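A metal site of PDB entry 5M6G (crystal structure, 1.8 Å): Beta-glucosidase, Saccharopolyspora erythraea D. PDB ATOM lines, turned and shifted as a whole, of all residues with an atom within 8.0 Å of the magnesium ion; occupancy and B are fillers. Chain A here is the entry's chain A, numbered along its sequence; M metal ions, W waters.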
ATOM      1  N   VAL A 184     -18.483  -6.762   7.922  1.00  0.00           N
ATOM      2  CA  VAL A 184     -18.815  -7.239   9.264  1.00  0.00           C
ATOM      3  C   VAL A 184     -18.045  -8.542   9.446  1.00  0.00           C
ATOM      4  O   VAL A 184     -18.443  -9.588   8.916  1.00  0.00           O
ATOM      5  CB  VAL A 184     -20.319  -7.439   9.427  1.00  0.00           C
ATOM      6  CG1 VAL A 184     -20.637  -7.967  10.795  1.00  0.00           C
ATOM      7  CG2 VAL A 184     -21.052  -6.126   9.167  1.00  0.00           C
ATOM      8  N   ALA A 185     -16.945  -8.492  10.198  1.00  0.00           N
ATOM      9  CA  ALA A 185     -16.041  -9.635  10.291  1.00  0.00           C
ATOM     10  C   ALA A 185     -16.595 -10.628  11.316  1.00  0.00           C
ATOM     11  O   ALA A 185     -16.632 -10.338  12.512  1.00  0.00           O
ATOM     12  CB  ALA A 185     -14.638  -9.175  10.682  1.00  0.00           C
ATOM     13  N   ARG A 186     -16.998 -11.806  10.830  1.00  0.00           N
ATOM     14  CA  ARG A 186     -17.582 -12.835  11.684  1.00  0.00           C
ATOM     15  C   ARG A 186     -16.622 -13.975  12.018  1.00  0.00           C
ATOM     16  O   ARG A 186     -16.968 -14.826  12.831  1.00  0.00           O
ATOM     17  CB  ARG A 186     -18.831 -13.433  11.015  1.00  0.00           C
ATOM     18  CG  ARG A 186     -19.832 -12.401  10.527  1.00  0.00           C
ATOM     19  CD  ARG A 186     -20.672 -11.857  11.665  1.00  0.00           C
ATOM     20  NE  ARG A 186     -21.601 -12.862  12.192  1.00  0.00           N
ATOM     21  CZ  ARG A 186     -22.301 -12.676  13.315  1.00  0.00           C
ATOM     22  NH1 ARG A 186     -23.137 -13.617  13.755  1.00  0.00           N
ATOM     23  NH2 ARG A 186     -22.166 -11.550  13.999  1.00  0.00           N
ATOM     24  N   ASP A 187     -15.440 -14.021  11.404  1.00  0.00           N
ATOM     25  CA  ASP A 187     -14.486 -15.099  11.657  1.00  0.00           C
ATOM     26  C   ASP A 187     -13.076 -14.531  11.795  1.00  0.00           C
ATOM     27  O   ASP A 187     -12.463 -14.125  10.794  1.00  0.00           O
ATOM     28  CB  ASP A 187     -14.545 -16.159  10.550  1.00  0.00           C
ATOM     29  CG  ASP A 187     -13.866 -17.457  10.947  1.00  0.00           C
ATOM     30  OD1 ASP A 187     -12.711 -17.406  11.416  1.00  0.00           O
ATOM     31  OD2 ASP A 187     -14.481 -18.536  10.773  1.00  0.00           O
ATOM     32  N   ASP A 188     -12.549 -14.541  13.013  1.00  0.00           N
ATOM     33  CA  ASP A 188     -11.292 -13.858  13.315  1.00  0.00           C
ATOM     34  C   ASP A 188     -10.115 -14.416  12.524  1.00  0.00           C
ATOM     35  O   ASP A 188      -9.064 -13.767  12.475  1.00  0.00           O
ATOM     36  CB  ASP A 188     -11.000 -13.939  14.814  1.00  0.00           C
ATOM     37  CG  ASP A 188     -11.913 -13.056  15.632  1.00  0.00           C
ATOM     38  OD1 ASP A 188     -12.641 -12.232  15.028  1.00  0.00           O
ATOM     39  OD2 ASP A 188     -11.886 -13.169  16.877  1.00  0.00           O
ATOM     40  N   THR A 193      -9.850  -8.959   9.296  1.00  0.00           N
ATOM     41  CA  THR A 193     -10.633  -8.685  10.493  1.00  0.00           C
ATOM     42  C   THR A 193     -10.357  -7.281  11.016  1.00  0.00           C
ATOM     43  O   THR A 193     -11.269  -6.602  11.497  1.00  0.00           O
ATOM     44  CB  THR A 193     -10.326  -9.743  11.562  1.00  0.00           C
ATOM     45  OG1 THR A 193     -10.756 -11.025  11.088  1.00  0.00           O
ATOM     46  CG2 THR A 193     -11.056  -9.416  12.869  1.00  0.00           C
ATOM     47  N   GLY A 198     -16.393  -4.151  13.381  1.00  0.00           N
ATOM     48  CA  GLY A 198     -16.865  -5.053  14.407  1.00  0.00           C
ATOM     49  C   GLY A 198     -17.674  -6.178  13.821  1.00  0.00           C
ATOM     50  O   GLY A 198     -18.022  -6.191  12.645  1.00  0.00           O
ATOM     51  N   GLU A 199     -17.996  -7.148  14.683  1.00  0.00           N
ATOM     52  CA  GLU A 199     -18.706  -8.336  14.263  1.00  0.00           C
ATOM     53  C   GLU A 199     -20.210  -8.134  14.160  1.00  0.00           C
ATOM     54  O   GLU A 199     -20.902  -9.007  13.615  1.00  0.00           O
ATOM     55  CB  GLU A 199     -18.423  -9.497  15.224  1.00  0.00           C
ATOM     56  CG  GLU A 199     -19.168  -9.367  16.531  1.00  0.00           C
ATOM     57  CD  GLU A 199     -18.772 -10.440  17.550  1.00  0.00           C
ATOM     58  OE1 GLU A 199     -17.712 -11.079  17.361  1.00  0.00           O
ATOM     59  OE2 GLU A 199     -19.530 -10.629  18.524  1.00  0.00           O
ATOM     60  N   LYS A 200     -20.744  -7.039  14.700  1.00  0.00           N
ATOM     61  CA  LYS A 200     -22.173  -6.795  14.688  1.00  0.00           C
ATOM     62  C   LYS A 200     -22.511  -5.722  13.667  1.00  0.00           C
ATOM     63  O   LYS A 200     -21.808  -4.711  13.570  1.00  0.00           O
ATOM     64  CB  LYS A 200     -22.685  -6.371  16.068  1.00  0.00           C
ATOM     65  CG  LYS A 200     -22.507  -7.448  17.122  1.00  0.00           C
ATOM     66  CD  LYS A 200     -22.990  -6.977  18.481  1.00  0.00           C
ATOM     67  CE  LYS A 200     -24.493  -6.880  18.542  1.00  0.00           C
ATOM     68  NZ  LYS A 200     -25.065  -8.127  19.074  1.00  0.00           N
ATOM     69  N   PRO A 543      -8.819 -10.419  18.081  1.00  0.00           N
ATOM     70  CA  PRO A 543      -8.538 -11.224  19.271  1.00  0.00           C
ATOM     71  C   PRO A 543      -7.486 -12.281  18.959  1.00  0.00           C
ATOM     72  O   PRO A 543      -7.402 -12.783  17.843  1.00  0.00           O
ATOM     73  CB  PRO A 543      -9.899 -11.858  19.594  1.00  0.00           C
ATOM     74  CG  PRO A 543     -10.912 -10.905  18.980  1.00  0.00           C
ATOM     75  CD  PRO A 543     -10.243 -10.413  17.717  1.00  0.00           C
ATOM     76  N   PRO A 584     -15.232  -4.853  20.199  1.00  0.00           N
ATOM     77  CA  PRO A 584     -16.085  -4.917  19.014  1.00  0.00           C
ATOM     78  C   PRO A 584     -16.217  -6.310  18.421  1.00  0.00           C
ATOM     79  O   PRO A 584     -17.063  -6.512  17.532  1.00  0.00           O
ATOM     80  CB  PRO A 584     -15.362  -3.976  18.031  1.00  0.00           C
ATOM     81  CG  PRO A 584     -13.905  -4.194  18.379  1.00  0.00           C
ATOM     82  CD  PRO A 584     -13.872  -4.342  19.889  1.00  0.00           C
ATOM     83  N   MET A 585     -15.386  -7.260  18.842  1.00  0.00           N
ATOM     84  CA  MET A 585     -15.507  -8.669  18.491  1.00  0.00           C
ATOM     85  C   MET A 585     -15.556  -9.478  19.773  1.00  0.00           C
ATOM     86  O   MET A 585     -14.951  -9.101  20.781  1.00  0.00           O
ATOM     87  CB  MET A 585     -14.319  -9.185  17.631  1.00  0.00           C
ATOM     88  CG  MET A 585     -14.352  -8.855  16.117  1.00  0.00           C
ATOM     89  SD  MET A 585     -14.171  -7.095  15.807  1.00  0.00           S
ATOM     90  CE  MET A 585     -13.822  -6.995  14.047  1.00  0.00           C
ATOM     91  N   THR A 586     -16.281 -10.590  19.738  1.00  0.00           N
ATOM     92  CA  THR A 586     -16.286 -11.532  20.846  1.00  0.00           C
ATOM     93  C   THR A 586     -14.925 -12.244  20.934  1.00  0.00           C
ATOM     94  O   THR A 586     -14.379 -12.687  19.918  1.00  0.00           O
ATOM     95  CB  THR A 586     -17.414 -12.550  20.654  1.00  0.00           C
ATOM     96  OG1 THR A 586     -18.672 -11.881  20.709  1.00  0.00           O
ATOM     97  CG2 THR A 586     -17.378 -13.603  21.727  1.00  0.00           C
ATOM     98  N   TRP A 587     -14.379 -12.354  22.136  1.00  0.00           N
ATOM     99  CA  TRP A 587     -13.019 -12.872  22.325  1.00  0.00           C
ATOM    100  C   TRP A 587     -13.060 -14.345  22.710  1.00  0.00           C
ATOM    101  O   TRP A 587     -13.615 -14.704  23.764  1.00  0.00           O
ATOM    102  CB  TRP A 587     -12.284 -12.058  23.388  1.00  0.00           C
ATOM    103  CG  TRP A 587     -10.796 -12.214  23.341  1.00  0.00           C
ATOM    104  CD1 TRP A 587     -10.079 -13.369  23.508  1.00  0.00           C
ATOM    105  CD2 TRP A 587      -9.834 -11.175  23.118  1.00  0.00           C
ATOM    106  NE1 TRP A 587      -8.723 -13.107  23.396  1.00  0.00           N
ATOM    107  CE2 TRP A 587      -8.553 -11.762  23.152  1.00  0.00           C
ATOM    108  CE3 TRP A 587      -9.932  -9.791  22.882  1.00  0.00           C
ATOM    109  CZ2 TRP A 587      -7.380 -11.035  22.967  1.00  0.00           C
ATOM    110  CZ3 TRP A 587      -8.759  -9.065  22.697  1.00  0.00           C
ATOM    111  CH2 TRP A 587      -7.504  -9.684  22.737  1.00  0.00           C
ATOM    112  N   MET A 588     -12.415 -15.189  21.901  1.00  0.00           N
ATOM    113  CA  MET A 588     -12.528 -16.639  22.026  1.00  0.00           C
ATOM    114  C   MET A 588     -11.912 -17.165  23.335  1.00  0.00           C
ATOM    115  O   MET A 588     -10.893 -16.658  23.826  1.00  0.00           O
ATOM    116  CB  MET A 588     -11.828 -17.308  20.844  1.00  0.00           C
ATOM    117  CG  MET A 588     -10.294 -17.213  20.916  1.00  0.00           C
ATOM    118  SD  MET A 588      -9.408 -17.593  19.406  1.00  0.00           S
ATOM    119  CE  MET A 588      -9.177 -15.945  18.728  1.00  0.00           C
ATOM    120  N   LEU A 594     -13.974 -20.583  16.832  1.00  0.00           N
ATOM    121  CA  LEU A 594     -14.152 -19.737  15.658  1.00  0.00           C
ATOM    122  C   LEU A 594     -14.988 -20.478  14.611  1.00  0.00           C
ATOM    123  O   LEU A 594     -14.798 -21.677  14.396  1.00  0.00           O
ATOM    124  CB  LEU A 594     -12.804 -19.318  15.066  1.00  0.00           C
ATOM    125  CG  LEU A 594     -11.878 -18.608  16.036  1.00  0.00           C
ATOM    126  CD1 LEU A 594     -10.691 -18.053  15.263  1.00  0.00           C
ATOM    127  CD2 LEU A 594     -12.637 -17.510  16.763  1.00  0.00           C
ATOM    128  N   PRO A 595     -15.925 -19.773  13.957  1.00  0.00           N
ATOM    129  CA  PRO A 595     -16.274 -18.358  14.222  1.00  0.00           C
ATOM    130  C   PRO A 595     -17.085 -18.190  15.509  1.00  0.00           C
ATOM    131  O   PRO A 595     -17.994 -18.992  15.760  1.00  0.00           O
ATOM    132  CB  PRO A 595     -17.117 -17.982  13.006  1.00  0.00           C
ATOM    133  CG  PRO A 595     -17.772 -19.290  12.613  1.00  0.00           C
ATOM    134  CD  PRO A 595     -16.712 -20.330  12.839  1.00  0.00           C
ATOM    135  N   ILE A 596     -16.767 -17.172  16.321  1.00  0.00           N
ATOM    136  CA  ILE A 596     -17.523 -16.897  17.538  1.00  0.00           C
ATOM    137  C   ILE A 596     -18.096 -15.485  17.449  1.00  0.00           C
ATOM    138  O   ILE A 596     -17.383 -14.541  17.096  1.00  0.00           O
ATOM    139  CB  ILE A 596     -16.671 -17.087  18.810  1.00  0.00           C
ATOM    140  CG1 ILE A 596     -17.548 -16.903  20.059  1.00  0.00           C
ATOM    141  CG2 ILE A 596     -15.443 -16.159  18.811  1.00  0.00           C
ATOM    142  CD1 ILE A 596     -16.913 -17.421  21.338  1.00  0.00           C
ATOM    143  N   ASN A 597     -19.381 -15.359  17.737  1.00  0.00           N
ATOM    144  CA  ASN A 597     -20.049 -14.076  17.584  1.00  0.00           C
ATOM    145  C   ASN A 597     -21.127 -13.936  18.634  1.00  0.00           C
ATOM    146  O   ASN A 597     -21.725 -14.926  19.077  1.00  0.00           O
ATOM    147  CB  ASN A 597     -20.658 -13.927  16.189  1.00  0.00           C
ATOM    148  CG  ASN A 597     -19.603 -13.909  15.111  1.00  0.00           C
ATOM    149  OD1 ASN A 597     -18.959 -12.891  14.902  1.00  0.00           O
ATOM    150  ND2 ASN A 597     -19.425 -15.035  14.436  1.00  0.00           N
ATOM    151  N   ASP A 598     -21.372 -12.697  19.020  1.00  0.00           N
ATOM    152  CA  ASP A 598     -22.378 -12.361  20.014  1.00  0.00           C
ATOM    153  C   ASP A 598     -23.703 -13.033  19.682  1.00  0.00           C
ATOM    154  O   ASP A 598     -24.175 -12.978  18.540  1.00  0.00           O
ATOM    155  CB  ASP A 598     -22.553 -10.842  20.068  1.00  0.00           C
ATOM    156  CG  ASP A 598     -23.227 -10.376  21.333  1.00  0.00           C
ATOM    157  OD1 ASP A 598     -22.881 -10.890  22.413  1.00  0.00           O
ATOM    158  OD2 ASP A 598     -24.113  -9.499  21.253  1.00  0.00           O
ATOM    159  N   ASP A 600     -24.332 -16.309  19.646  1.00  0.00           N
ATOM    160  CA  ASP A 600     -24.280 -17.642  19.073  1.00  0.00           C
ATOM    161  C   ASP A 600     -24.299 -18.746  20.132  1.00  0.00           C
ATOM    162  O   ASP A 600     -24.142 -19.921  19.771  1.00  0.00           O
ATOM    163  CB  ASP A 600     -23.055 -17.807  18.164  1.00  0.00           C
ATOM    164  CG  ASP A 600     -21.731 -17.846  18.936  1.00  0.00           C
ATOM    165  OD1 ASP A 600     -21.722 -17.790  20.192  1.00  0.00           O
ATOM    166  OD2 ASP A 600     -20.682 -17.939  18.242  1.00  0.00           O
ATOM    167  N   HIS A 608     -18.629  -9.588  23.553  1.00  0.00           N
ATOM    168  CA  HIS A 608     -18.796  -8.337  22.827  1.00  0.00           C
ATOM    169  C   HIS A 608     -19.262  -7.241  23.782  1.00  0.00           C
ATOM    170  O   HIS A 608     -20.105  -7.467  24.641  1.00  0.00           O
ATOM    171  CB  HIS A 608     -19.822  -8.553  21.704  1.00  0.00           C
ATOM    172  CG  HIS A 608     -19.974  -7.377  20.795  1.00  0.00           C
ATOM    173  ND1 HIS A 608     -20.692  -6.247  21.141  1.00  0.00           N
ATOM    174  CD2 HIS A 608     -19.486  -7.148  19.549  1.00  0.00           C
ATOM    175  CE1 HIS A 608     -20.633  -5.370  20.147  1.00  0.00           C
ATOM    176  NE2 HIS A 608     -19.922  -5.900  19.169  1.00  0.00           N
HETATM  177 MG    MG M   1     -16.834 -12.548  16.055  1.00  0.00          MG
HETATM  178  O   HOH W   1     -14.882 -12.755  17.231  1.00  0.00           O
HETATM  179  O   HOH W   2     -14.989 -15.178  15.052  1.00  0.00           O
HETATM  180  O   HOH W   3     -15.639 -11.829  14.341  1.00  0.00           O
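The side-chain amide nitrogen of Asn 597 sits at hydrogen-bond distance from the backbone carbonyl oxygen of Arg 186 (2.9 Å).
The backbone carbonyl oxygen (O) of Glu 199 lies within hydrogen-bond range of the guanidinium group (NH2) of Arg 186, at 2.9 Å.
The backbone NH (N) of Glu 199 is in hydrogen-bond range of the backbone carbonyl oxygen (O) of Pro 584.
OE2 of Glu 199 is in hydrogen-bond range of N of Asp 598 (2.8 Å).
OG1 of Thr 586 sits at hydrogen-bond distance from OE2 of Glu 199, at 2.7 Å.
N of Asn 597 lies within hydrogen-bond range of OD2 of Asp 600 (2.9 Å).
Arg 186 touches the magnesium ion.
Four residues have an atom within 4 Å of the magnesium ion: Arg 186, Glu 199, Ile 596 and Asn 597.
The magnesium ion is bound by OE1 of Glu 199 (2.2 Å).
The magnesium ion is bound by water W3, 2.2 Å away.
Water W1 binds the magnesium ion (2.3 Å).
The magnesium ion is bound by O of Ile 596 (2.3 Å).
The side-chain amide oxygen (OD1) of Asn 597 binds the magnesium ion, at 2.4 Å.
Water W3 lies within hydrogen-bond range of O of Ala 185 (2.6 Å) and OD1 of Asp 188 (3.1 Å).
Water W1 bridges O of Thr 586 (2.7 Å) and OD2 of Asp 188 (3.0 Å).
Water W2 lies within hydrogen-bond range of N of Ile 596 (3.0 Å), O of Arg 186 (3.0 Å) and N of Asp 188 (3.2 Å).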
